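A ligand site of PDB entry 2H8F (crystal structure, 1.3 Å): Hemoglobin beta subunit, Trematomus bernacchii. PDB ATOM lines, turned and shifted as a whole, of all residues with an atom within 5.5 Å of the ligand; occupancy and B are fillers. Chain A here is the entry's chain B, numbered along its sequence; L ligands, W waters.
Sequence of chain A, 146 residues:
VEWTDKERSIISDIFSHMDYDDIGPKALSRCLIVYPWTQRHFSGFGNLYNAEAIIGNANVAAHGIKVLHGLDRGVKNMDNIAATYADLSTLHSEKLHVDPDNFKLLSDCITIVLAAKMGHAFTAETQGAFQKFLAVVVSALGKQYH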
ATOM      1  N   LEU A  32     -15.920  -6.673 -20.299  1.00  0.00           N
ATOM      2  CA  LEU A  32     -16.554  -6.528 -18.997  1.00  0.00           C
ATOM      3  C   LEU A  32     -16.511  -5.110 -18.493  1.00  0.00           C
ATOM      4  O   LEU A  32     -17.371  -4.771 -17.630  1.00  0.00           O
ATOM      5  CB  LEU A  32     -15.870  -7.508 -18.029  1.00  0.00           C
ATOM      6  CG  LEU A  32     -15.853  -8.981 -18.363  1.00  0.00           C
ATOM      7  CD1 LEU A  32     -15.303  -9.827 -17.212  1.00  0.00           C
ATOM      8  CD2 LEU A  32     -17.236  -9.501 -18.723  1.00  0.00           C
ATOM      9  N   THR A  38     -22.150  -7.643 -19.529  1.00  0.00           N
ATOM     10  CA  THR A  38     -21.558  -8.943 -19.987  1.00  0.00           C
ATOM     11  C   THR A  38     -21.013  -9.669 -18.774  1.00  0.00           C
ATOM     12  O   THR A  38     -20.695 -10.865 -18.897  1.00  0.00           O
ATOM     13  CB  THR A  38     -20.514  -8.745 -21.080  1.00  0.00           C
ATOM     14  OG1 THR A  38     -19.428  -7.929 -20.642  1.00  0.00           O
ATOM     15  CG2 THR A  38     -21.219  -8.147 -22.311  1.00  0.00           C
ATOM     16  N   HIS A  41     -22.814 -13.506 -16.506  1.00  0.00           N
ATOM     17  CA  HIS A  41     -22.433 -14.919 -16.441  1.00  0.00           C
ATOM     18  C   HIS A  41     -21.262 -15.317 -15.572  1.00  0.00           C
ATOM     19  O   HIS A  41     -21.026 -16.550 -15.439  1.00  0.00           O
ATOM     20  CB  HIS A  41     -21.999 -15.310 -17.895  1.00  0.00           C
ATOM     21  CG  HIS A  41     -23.093 -14.791 -18.776  1.00  0.00           C
ATOM     22  ND1 HIS A  41     -24.320 -15.452 -18.806  1.00  0.00           N
ATOM     23  CD2 HIS A  41     -23.172 -13.679 -19.565  1.00  0.00           C
ATOM     24  CE1 HIS A  41     -25.095 -14.776 -19.624  1.00  0.00           C
ATOM     25  NE2 HIS A  41     -24.433 -13.720 -20.096  1.00  0.00           N
ATOM     26  N   PHE A  42     -20.532 -14.373 -15.028  1.00  0.00           N
ATOM     27  CA  PHE A  42     -19.253 -14.558 -14.363  1.00  0.00           C
ATOM     28  C   PHE A  42     -19.226 -14.271 -12.862  1.00  0.00           C
ATOM     29  O   PHE A  42     -18.144 -14.024 -12.342  1.00  0.00           O
ATOM     30  CB  PHE A  42     -18.182 -13.689 -15.071  1.00  0.00           C
ATOM     31  CG  PHE A  42     -18.165 -13.995 -16.561  1.00  0.00           C
ATOM     32  CD1 PHE A  42     -17.846 -15.264 -17.009  1.00  0.00           C
ATOM     33  CD2 PHE A  42     -18.448 -13.054 -17.534  1.00  0.00           C
ATOM     34  CE1 PHE A  42     -17.820 -15.606 -18.352  1.00  0.00           C
ATOM     35  CE2 PHE A  42     -18.395 -13.388 -18.860  1.00  0.00           C
ATOM     36  CZ  PHE A  42     -18.057 -14.632 -19.302  1.00  0.00           C
ATOM     37  N   PHE A  45     -16.405 -15.842 -10.772  1.00  0.00           N
ATOM     38  CA  PHE A  45     -15.025 -15.537 -11.110  1.00  0.00           C
ATOM     39  C   PHE A  45     -14.370 -14.731 -10.024  1.00  0.00           C
ATOM     40  O   PHE A  45     -13.187 -14.385 -10.073  1.00  0.00           O
ATOM     41  CB  PHE A  45     -15.087 -14.751 -12.428  1.00  0.00           C
ATOM     42  CG  PHE A  45     -15.108 -15.705 -13.610  1.00  0.00           C
ATOM     43  CD1 PHE A  45     -15.804 -16.882 -13.520  1.00  0.00           C
ATOM     44  CD2 PHE A  45     -14.433 -15.372 -14.765  1.00  0.00           C
ATOM     45  CE1 PHE A  45     -15.879 -17.801 -14.540  1.00  0.00           C
ATOM     46  CE2 PHE A  45     -14.507 -16.279 -15.825  1.00  0.00           C
ATOM     47  CZ  PHE A  45     -15.195 -17.479 -15.715  1.00  0.00           C
ATOM     48  N   HIS A  63     -10.559 -17.240 -18.882  1.00  0.00           N
ATOM     49  CA  HIS A  63     -11.724 -17.485 -19.734  1.00  0.00           C
ATOM     50  C   HIS A  63     -11.542 -16.732 -21.040  1.00  0.00           C
ATOM     51  O   HIS A  63     -11.992 -17.164 -22.115  1.00  0.00           O
ATOM     52  CB  HIS A  63     -12.982 -17.019 -19.037  1.00  0.00           C
ATOM     53  CG  HIS A  63     -14.205 -17.420 -19.768  1.00  0.00           C
ATOM     54  ND1 HIS A  63     -14.667 -18.718 -19.778  1.00  0.00           N
ATOM     55  CD2 HIS A  63     -15.101 -16.701 -20.517  1.00  0.00           C
ATOM     56  CE1 HIS A  63     -15.767 -18.803 -20.478  1.00  0.00           C
ATOM     57  NE2 HIS A  63     -16.061 -17.600 -20.953  1.00  0.00           N
ATOM     58  N   LYS A  66      -9.623 -18.994 -23.317  1.00  0.00           N
ATOM     59  CA  LYS A  66     -10.527 -20.033 -23.793  1.00  0.00           C
ATOM     60  C   LYS A  66     -11.483 -19.588 -24.900  1.00  0.00           C
ATOM     61  O   LYS A  66     -11.597 -20.163 -25.943  1.00  0.00           O
ATOM     62  CB  LYS A  66     -11.370 -20.575 -22.641  1.00  0.00           C
ATOM     63  CG  LYS A  66     -12.096 -21.902 -22.992  1.00  0.00           C
ATOM     64  CD  LYS A  66     -12.994 -22.292 -21.817  1.00  0.00           C
ATOM     65  CE  LYS A  66     -12.181 -22.627 -20.593  1.00  0.00           C
ATOM     66  NZ  LYS A  66     -13.043 -23.245 -19.508  1.00  0.00           N
ATOM     67  N   VAL A  67     -12.172 -18.462 -24.641  1.00  0.00           N
ATOM     68  CA  VAL A  67     -12.988 -17.920 -25.704  1.00  0.00           C
ATOM     69  C   VAL A  67     -12.224 -17.586 -26.944  1.00  0.00           C
ATOM     70  O   VAL A  67     -12.654 -17.842 -28.114  1.00  0.00           O
ATOM     71  CB  VAL A  67     -13.718 -16.677 -25.102  1.00  0.00           C
ATOM     72  CG1 VAL A  67     -14.341 -15.912 -26.238  1.00  0.00           C
ATOM     73  CG2 VAL A  67     -14.655 -17.238 -24.037  1.00  0.00           C
ATOM     74  N   GLY A  70     -11.585 -20.522 -28.890  1.00  0.00           N
ATOM     75  CA  GLY A  70     -12.773 -21.095 -29.498  1.00  0.00           C
ATOM     76  C   GLY A  70     -12.922 -20.569 -30.930  1.00  0.00           C
ATOM     77  O   GLY A  70     -13.748 -21.148 -31.667  1.00  0.00           O
ATOM     78  N   LEU A  71     -12.231 -19.546 -31.378  1.00  0.00           N
ATOM     79  CA  LEU A  71     -12.229 -19.176 -32.763  1.00  0.00           C
ATOM     80  C   LEU A  71     -11.436 -20.146 -33.612  1.00  0.00           C
ATOM     81  O   LEU A  71     -11.615 -20.116 -34.823  1.00  0.00           O
ATOM     82  CB  LEU A  71     -11.692 -17.745 -32.891  1.00  0.00           C
ATOM     83  CG  LEU A  71     -12.463 -16.639 -32.129  1.00  0.00           C
ATOM     84  CD1 LEU A  71     -11.747 -15.304 -32.290  1.00  0.00           C
ATOM     85  CD2 LEU A  71     -13.891 -16.647 -32.649  1.00  0.00           C
ATOM     86  N   ARG A  73     -11.346 -23.365 -34.294  1.00  0.00           N
ATOM     87  CA  ARG A  73     -12.154 -24.301 -35.115  1.00  0.00           C
ATOM     88  C   ARG A  73     -12.784 -23.605 -36.301  1.00  0.00           C
ATOM     89  O   ARG A  73     -13.001 -24.251 -37.321  1.00  0.00           O
ATOM     90  CB  ARG A  73     -13.239 -24.958 -34.329  1.00  0.00           C
ATOM     91  CG  ARG A  73     -14.340 -24.009 -33.815  1.00  0.00           C
ATOM     92  CD  ARG A  73     -15.097 -24.782 -32.755  1.00  0.00           C
ATOM     93  NE  ARG A  73     -14.538 -24.754 -31.405  1.00  0.00           N
ATOM     94  CZ  ARG A  73     -14.929 -25.475 -30.358  1.00  0.00           C
ATOM     95  NH1 ARG A  73     -15.910 -26.355 -30.411  1.00  0.00           N
ATOM     96  NH2 ARG A  73     -14.319 -25.339 -29.189  1.00  0.00           N
ATOM     97  N   TYR A  85     -19.915 -24.641 -35.182  1.00  0.00           N
ATOM     98  CA  TYR A  85     -20.312 -24.049 -33.904  1.00  0.00           C
ATOM     99  C   TYR A  85     -21.683 -24.408 -33.370  1.00  0.00           C
ATOM    100  O   TYR A  85     -22.101 -23.822 -32.343  1.00  0.00           O
ATOM    101  CB  TYR A  85     -20.235 -22.479 -33.993  1.00  0.00           C
ATOM    102  CG  TYR A  85     -18.784 -22.032 -34.006  1.00  0.00           C
ATOM    103  CD1 TYR A  85     -18.107 -21.769 -32.820  1.00  0.00           C
ATOM    104  CD2 TYR A  85     -18.108 -21.873 -35.212  1.00  0.00           C
ATOM    105  CE1 TYR A  85     -16.801 -21.368 -32.854  1.00  0.00           C
ATOM    106  CE2 TYR A  85     -16.761 -21.457 -35.236  1.00  0.00           C
ATOM    107  CZ  TYR A  85     -16.159 -21.228 -34.049  1.00  0.00           C
ATOM    108  OH  TYR A  85     -14.839 -20.809 -33.972  1.00  0.00           O
ATOM    109  N   LEU A  88     -21.545 -25.548 -29.619  1.00  0.00           N
ATOM    110  CA  LEU A  88     -21.282 -24.352 -28.807  1.00  0.00           C
ATOM    111  C   LEU A  88     -22.503 -23.387 -28.724  1.00  0.00           C
ATOM    112  O   LEU A  88     -22.715 -22.826 -27.666  1.00  0.00           O
ATOM    113  CB  LEU A  88     -20.056 -23.577 -29.335  1.00  0.00           C
ATOM    114  CG  LEU A  88     -18.733 -24.048 -28.691  1.00  0.00           C
ATOM    115  CD1 LEU A  88     -17.548 -23.321 -29.317  1.00  0.00           C
ATOM    116  CD2 LEU A  88     -18.794 -23.931 -27.164  1.00  0.00           C
ATOM    117  N   LEU A  91     -24.886 -24.983 -26.343  1.00  0.00           N
ATOM    118  CA  LEU A  91     -24.401 -24.822 -24.984  1.00  0.00           C
ATOM    119  C   LEU A  91     -24.674 -23.406 -24.430  1.00  0.00           C
ATOM    120  O   LEU A  91     -25.200 -23.228 -23.327  1.00  0.00           O
ATOM    121  CB  LEU A  91     -22.906 -25.160 -24.971  1.00  0.00           C
ATOM    122  CG  LEU A  91     -22.270 -24.872 -23.582  1.00  0.00           C
ATOM    123  CD1 LEU A  91     -22.656 -25.974 -22.613  1.00  0.00           C
ATOM    124  CD2 LEU A  91     -20.761 -24.651 -23.697  1.00  0.00           C
ATOM    125  N   HIS A  92     -24.294 -22.421 -25.249  1.00  0.00           N
ATOM    126  CA  HIS A  92     -24.497 -21.021 -24.770  1.00  0.00           C
ATOM    127  C   HIS A  92     -25.935 -20.652 -24.550  1.00  0.00           C
ATOM    128  O   HIS A  92     -26.201 -19.851 -23.639  1.00  0.00           O
ATOM    129  CB  HIS A  92     -23.815 -20.058 -25.766  1.00  0.00           C
ATOM    130  CG  HIS A  92     -22.313 -19.956 -25.572  1.00  0.00           C
ATOM    131  ND1 HIS A  92     -21.445 -20.946 -26.054  1.00  0.00           N
ATOM    132  CD2 HIS A  92     -21.525 -19.090 -24.937  1.00  0.00           C
ATOM    133  CE1 HIS A  92     -20.173 -20.625 -25.727  1.00  0.00           C
ATOM    134  NE2 HIS A  92     -20.211 -19.475 -25.045  1.00  0.00           N
ATOM    135  N   LEU A  96     -25.963 -22.085 -20.602  1.00  0.00           N
ATOM    136  CA  LEU A  96     -25.306 -20.898 -20.092  1.00  0.00           C
ATOM    137  C   LEU A  96     -26.219 -19.653 -20.081  1.00  0.00           C
ATOM    138  O   LEU A  96     -25.997 -18.709 -19.327  1.00  0.00           O
ATOM    139  CB  LEU A  96     -24.091 -20.653 -21.004  1.00  0.00           C
ATOM    140  CG  LEU A  96     -22.972 -21.749 -20.983  1.00  0.00           C
ATOM    141  CD1 LEU A  96     -21.855 -21.390 -21.934  1.00  0.00           C
ATOM    142  CD2 LEU A  96     -22.382 -21.980 -19.585  1.00  0.00           C
ATOM    143  N   VAL A  98     -26.502 -17.244 -22.226  1.00  0.00           N
ATOM    144  CA  VAL A  98     -25.796 -16.006 -22.593  1.00  0.00           C
ATOM    145  C   VAL A  98     -26.599 -15.342 -23.690  1.00  0.00           C
ATOM    146  O   VAL A  98     -26.950 -15.882 -24.732  1.00  0.00           O
ATOM    147  CB  VAL A  98     -24.422 -16.320 -23.155  1.00  0.00           C
ATOM    148  CG1 VAL A  98     -23.754 -15.049 -23.645  1.00  0.00           C
ATOM    149  CG2 VAL A  98     -23.513 -16.953 -22.097  1.00  0.00           C
ATOM    150  N   ASN A 102     -24.206 -10.243 -26.750  1.00  0.00           N
ATOM    151  CA  ASN A 102     -22.923 -10.126 -26.065  1.00  0.00           C
ATOM    152  C   ASN A 102     -21.791 -10.699 -26.900  1.00  0.00           C
ATOM    153  O   ASN A 102     -20.640 -10.288 -26.705  1.00  0.00           O
ATOM    154  CB  ASN A 102     -22.946 -10.850 -24.713  1.00  0.00           C
ATOM    155  CG  ASN A 102     -23.842 -10.145 -23.684  1.00  0.00           C
ATOM    156  OD1 ASN A 102     -24.224 -10.772 -22.669  1.00  0.00           O
ATOM    157  ND2 ASN A 102     -24.136  -8.846 -23.893  1.00  0.00           N
ATOM    158  N   PHE A 103     -22.078 -11.624 -27.812  1.00  0.00           N
ATOM    159  CA  PHE A 103     -21.060 -12.147 -28.710  1.00  0.00           C
ATOM    160  C   PHE A 103     -20.538 -11.035 -29.574  1.00  0.00           C
ATOM    161  O   PHE A 103     -19.335 -10.917 -29.935  1.00  0.00           O
ATOM    162  CB  PHE A 103     -21.594 -13.258 -29.633  1.00  0.00           C
ATOM    163  CG  PHE A 103     -22.052 -14.492 -28.870  1.00  0.00           C
ATOM    164  CD1 PHE A 103     -21.396 -14.988 -27.799  1.00  0.00           C
ATOM    165  CD2 PHE A 103     -23.224 -15.100 -29.317  1.00  0.00           C
ATOM    166  CE1 PHE A 103     -21.849 -16.128 -27.103  1.00  0.00           C
ATOM    167  CE2 PHE A 103     -23.655 -16.232 -28.666  1.00  0.00           C
ATOM    168  CZ  PHE A 103     -23.007 -16.740 -27.567  1.00  0.00           C
ATOM    169  N   LEU A 106     -18.273  -8.602 -27.430  1.00  0.00           N
ATOM    170  CA  LEU A 106     -16.954  -9.174 -27.241  1.00  0.00           C
ATOM    171  C   LEU A 106     -16.191  -9.169 -28.534  1.00  0.00           C
ATOM    172  O   LEU A 106     -14.958  -8.872 -28.495  1.00  0.00           O
ATOM    173  CB  LEU A 106     -17.052 -10.604 -26.694  1.00  0.00           C
ATOM    174  CG  LEU A 106     -15.680 -11.259 -26.442  1.00  0.00           C
ATOM    175  CD1 LEU A 106     -14.827 -10.466 -25.441  1.00  0.00           C
ATOM    176  CD2 LEU A 106     -15.868 -12.724 -26.007  1.00  0.00           C
ATOM    177  N   SER A 107     -16.822  -9.441 -29.641  1.00  0.00           N
ATOM    178  CA  SER A 107     -16.166  -9.404 -30.960  1.00  0.00           C
ATOM    179  C   SER A 107     -15.537  -8.069 -31.219  1.00  0.00           C
ATOM    180  O   SER A 107     -14.391  -7.942 -31.710  1.00  0.00           O
ATOM    181  CB  SER A 107     -17.191  -9.718 -32.071  1.00  0.00           C
ATOM    182  OG  SER A 107     -17.392 -11.128 -32.138  1.00  0.00           O
ATOM    183  N   ILE A 110     -12.433  -7.759 -29.116  1.00  0.00           N
ATOM    184  CA  ILE A 110     -11.286  -8.501 -29.715  1.00  0.00           C
ATOM    185  C   ILE A 110     -10.745  -7.669 -30.819  1.00  0.00           C
ATOM    186  O   ILE A 110      -9.497  -7.486 -30.911  1.00  0.00           O
ATOM    187  CB  ILE A 110     -11.797  -9.886 -30.158  1.00  0.00           C
ATOM    188  CG1 ILE A 110     -12.195 -10.776 -28.999  1.00  0.00           C
ATOM    189  CG2 ILE A 110     -10.672 -10.581 -30.946  1.00  0.00           C
ATOM    190  CD1 ILE A 110     -12.965 -12.024 -29.552  1.00  0.00           C
ATOM    191  N   VAL A 137     -18.712 -16.218 -37.322  1.00  0.00           N
ATOM    192  CA  VAL A 137     -18.690 -16.978 -36.095  1.00  0.00           C
ATOM    193  C   VAL A 137     -19.796 -16.525 -35.174  1.00  0.00           C
ATOM    194  O   VAL A 137     -20.497 -17.330 -34.594  1.00  0.00           O
ATOM    195  CB  VAL A 137     -17.323 -16.890 -35.356  1.00  0.00           C
ATOM    196  CG1 VAL A 137     -17.417 -17.527 -34.003  1.00  0.00           C
ATOM    197  CG2 VAL A 137     -16.267 -17.538 -36.270  1.00  0.00           C
ATOM    198  N   VAL A 138     -19.985 -15.186 -35.009  1.00  0.00           N
ATOM    199  CA  VAL A 138     -21.056 -14.695 -34.123  1.00  0.00           C
ATOM    200  C   VAL A 138     -22.415 -15.143 -34.640  1.00  0.00           C
ATOM    201  O   VAL A 138     -23.254 -15.520 -33.813  1.00  0.00           O
ATOM    202  CB  VAL A 138     -20.959 -13.172 -33.998  1.00  0.00           C
ATOM    203  CG1 VAL A 138     -22.201 -12.519 -33.340  1.00  0.00           C
ATOM    204  CG2 VAL A 138     -19.666 -12.795 -33.199  1.00  0.00           C
ATOM    205  N   LEU A 141     -22.831 -18.743 -33.672  1.00  0.00           N
ATOM    206  CA  LEU A 141     -23.032 -18.874 -32.224  1.00  0.00           C
ATOM    207  C   LEU A 141     -24.461 -18.587 -31.792  1.00  0.00           C
ATOM    208  O   LEU A 141     -24.937 -19.111 -30.764  1.00  0.00           O
ATOM    209  CB  LEU A 141     -22.086 -17.944 -31.433  1.00  0.00           C
ATOM    210  CG  LEU A 141     -20.669 -18.549 -31.317  1.00  0.00           C
ATOM    211  CD1 LEU A 141     -19.719 -17.425 -30.891  1.00  0.00           C
ATOM    212  CD2 LEU A 141     -20.600 -19.726 -30.379  1.00  0.00           C
HETATM  213  C1  LIG L   1     -17.769 -21.225 -22.232  1.00  0.00           C
HETATM  214  C2  LIG L   1     -16.480 -19.998 -26.775  1.00  0.00           C
HETATM  215  C3  LIG L   1     -18.468 -15.609 -26.133  1.00  0.00           C
HETATM  216  C4  LIG L   1     -19.671 -16.818 -21.626  1.00  0.00           C
HETATM  217  C5  LIG L   1     -17.297 -21.312 -23.517  1.00  0.00           C
HETATM  218  C6  LIG L   1     -16.388 -22.333 -24.058  1.00  0.00           C
HETATM  219  C7  LIG L   1     -16.018 -21.966 -25.273  1.00  0.00           C
HETATM  220  C8  LIG L   1     -16.589 -20.635 -25.533  1.00  0.00           C
HETATM  221  C9  LIG L   1     -15.051 -22.590 -26.293  1.00  0.00           C
HETATM  222  C10 LIG L   1     -16.187 -23.701 -23.331  1.00  0.00           C
HETATM  223  C11 LIG L   1     -17.315 -24.690 -23.401  1.00  0.00           C
HETATM  224  C12 LIG L   1     -17.303 -25.878 -22.457  1.00  0.00           C
HETATM  225  O1  LIG L   1     -17.353 -26.995 -22.991  1.00  0.00           O
HETATM  226  O2  LIG L   1     -17.280 -25.642 -21.214  1.00  0.00           O
HETATM  227  C13 LIG L   1     -16.908 -18.692 -27.003  1.00  0.00           C
HETATM  228  C14 LIG L   1     -16.672 -17.900 -28.196  1.00  0.00           C
HETATM  229  C15 LIG L   1     -17.173 -16.684 -27.996  1.00  0.00           C
HETATM  230  C16 LIG L   1     -17.801 -16.712 -26.683  1.00  0.00           C
HETATM  231  C17 LIG L   1     -15.973 -18.445 -29.478  1.00  0.00           C
HETATM  232  C18 LIG L   1     -17.281 -15.463 -28.915  1.00  0.00           C
HETATM  233  C19 LIG L   1     -16.473 -15.214 -29.921  1.00  0.00           C
HETATM  234  C20 LIG L   1     -18.929 -15.573 -24.836  1.00  0.00           C
HETATM  235  C21 LIG L   1     -19.508 -14.383 -24.199  1.00  0.00           C
HETATM  236  C22 LIG L   1     -19.928 -14.731 -23.006  1.00  0.00           C
HETATM  237  C23 LIG L   1     -19.575 -16.147 -22.808  1.00  0.00           C
HETATM  238  C24 LIG L   1     -19.561 -13.010 -24.922  1.00  0.00           C
HETATM  239  C25 LIG L   1     -20.567 -13.931 -21.873  1.00  0.00           C
HETATM  240  C26 LIG L   1     -20.508 -12.595 -21.834  1.00  0.00           C
HETATM  241  C27 LIG L   1     -19.249 -18.125 -21.411  1.00  0.00           C
HETATM  242  C28 LIG L   1     -19.582 -18.871 -20.210  1.00  0.00           C
HETATM  243  C29 LIG L   1     -19.079 -20.123 -20.386  1.00  0.00           C
HETATM  244  C30 LIG L   1     -18.495 -20.178 -21.698  1.00  0.00           C
HETATM  245  C31 LIG L   1     -20.403 -18.318 -19.032  1.00  0.00           C
HETATM  246  C32 LIG L   1     -18.854 -21.162 -19.262  1.00  0.00           C
HETATM  247  C33 LIG L   1     -17.849 -20.745 -18.175  1.00  0.00           C
HETATM  248  C34 LIG L   1     -17.135 -21.906 -17.509  1.00  0.00           C
HETATM  249  O3  LIG L   1     -15.896 -21.829 -17.420  1.00  0.00           O
HETATM  250  O4  LIG L   1     -17.873 -22.845 -17.113  1.00  0.00           O
HETATM  251  N1  LIG L   1     -17.341 -20.272 -24.456  1.00  0.00           N
HETATM  252  N2  LIG L   1     -17.592 -17.917 -26.061  1.00  0.00           N
HETATM  253  N3  LIG L   1     -18.967 -16.613 -23.959  1.00  0.00           N
HETATM  254  N4  LIG L   1     -18.757 -18.977 -22.372  1.00  0.00           N
HETATM  255 FE1  LIG L   1     -18.399 -18.507 -24.315  1.00  0.00          FE
HETATM  256  O   HOH W   1     -13.378 -20.541 -18.272  1.00  0.00           O
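A ring nitrogen (NE2) of His 63 sits close to a nitrogen (N4) of the ligand, 3.3 Å away. O of Thr 38 touches C26 of the ligand (3.4 Å). CD2 of His 41 touches C25 of the ligand, 3.5 Å away. Phe 42 touches the ligand (CZ to C4, 3.6 Å). Val 67 touches the ligand (CG1 to C15, 3.4 Å). Gly 70 touches the ligand (C to C17, 3.99 Å). Leu 88 touches the ligand (CD2 to C7, 3.9 Å). Leu 91 touches the ligand. Leu 96 touches the ligand (CD1 to C29, 3.4 Å). CG1 of Val 98 touches C25 of the ligand (3.8 Å). Asn 102 touches the ligand (O to C24, 3.4 Å). Phe 103 touches the ligand (CD1 to C3, 3.4 Å). Leu 106 touches the ligand. Leu 141 touches the ligand. Hydrophobic or aromatic side chains within 4 Å of the ligand: His 41, Phe 42, His 63, Val 67, Leu 88, Leu 91, His 92, Leu 96, Val 98, Phe 103, Leu 106 and Leu 141. Of the 25 residues printed, 16 come within 4 Å of the ligand.
NE2 of His 92 is bound to FE1 of the ligand. An oxygen (O3) of the ligand lies within salt-bridge range of the side-chain amino group of Lys 66 (3.8 Å).
The backbone carbonyl oxygen of His 92 lies within hydrogen-bond range of the backbone NH of Val 98, 3.0 Å away. O of Leu 88 lies within hydrogen-bond range of ND1 of His 92. The backbone NH (N) of Leu 96 lies within hydrogen-bond range of the backbone carbonyl oxygen (O) of Leu 91, at 3.1 Å. O of Phe 103 lies within hydrogen-bond range of OG of Ser 107 (2.9 Å). O of Gly 70 sits at hydrogen-bond distance from OH of Tyr 85 (2.6 Å).
Water W1 lies within hydrogen-bond range of ND1 of His 63 (2.7 Å), O3 of the ligand (3.0 Å) and NZ of Lys 66 (3.0 Å).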
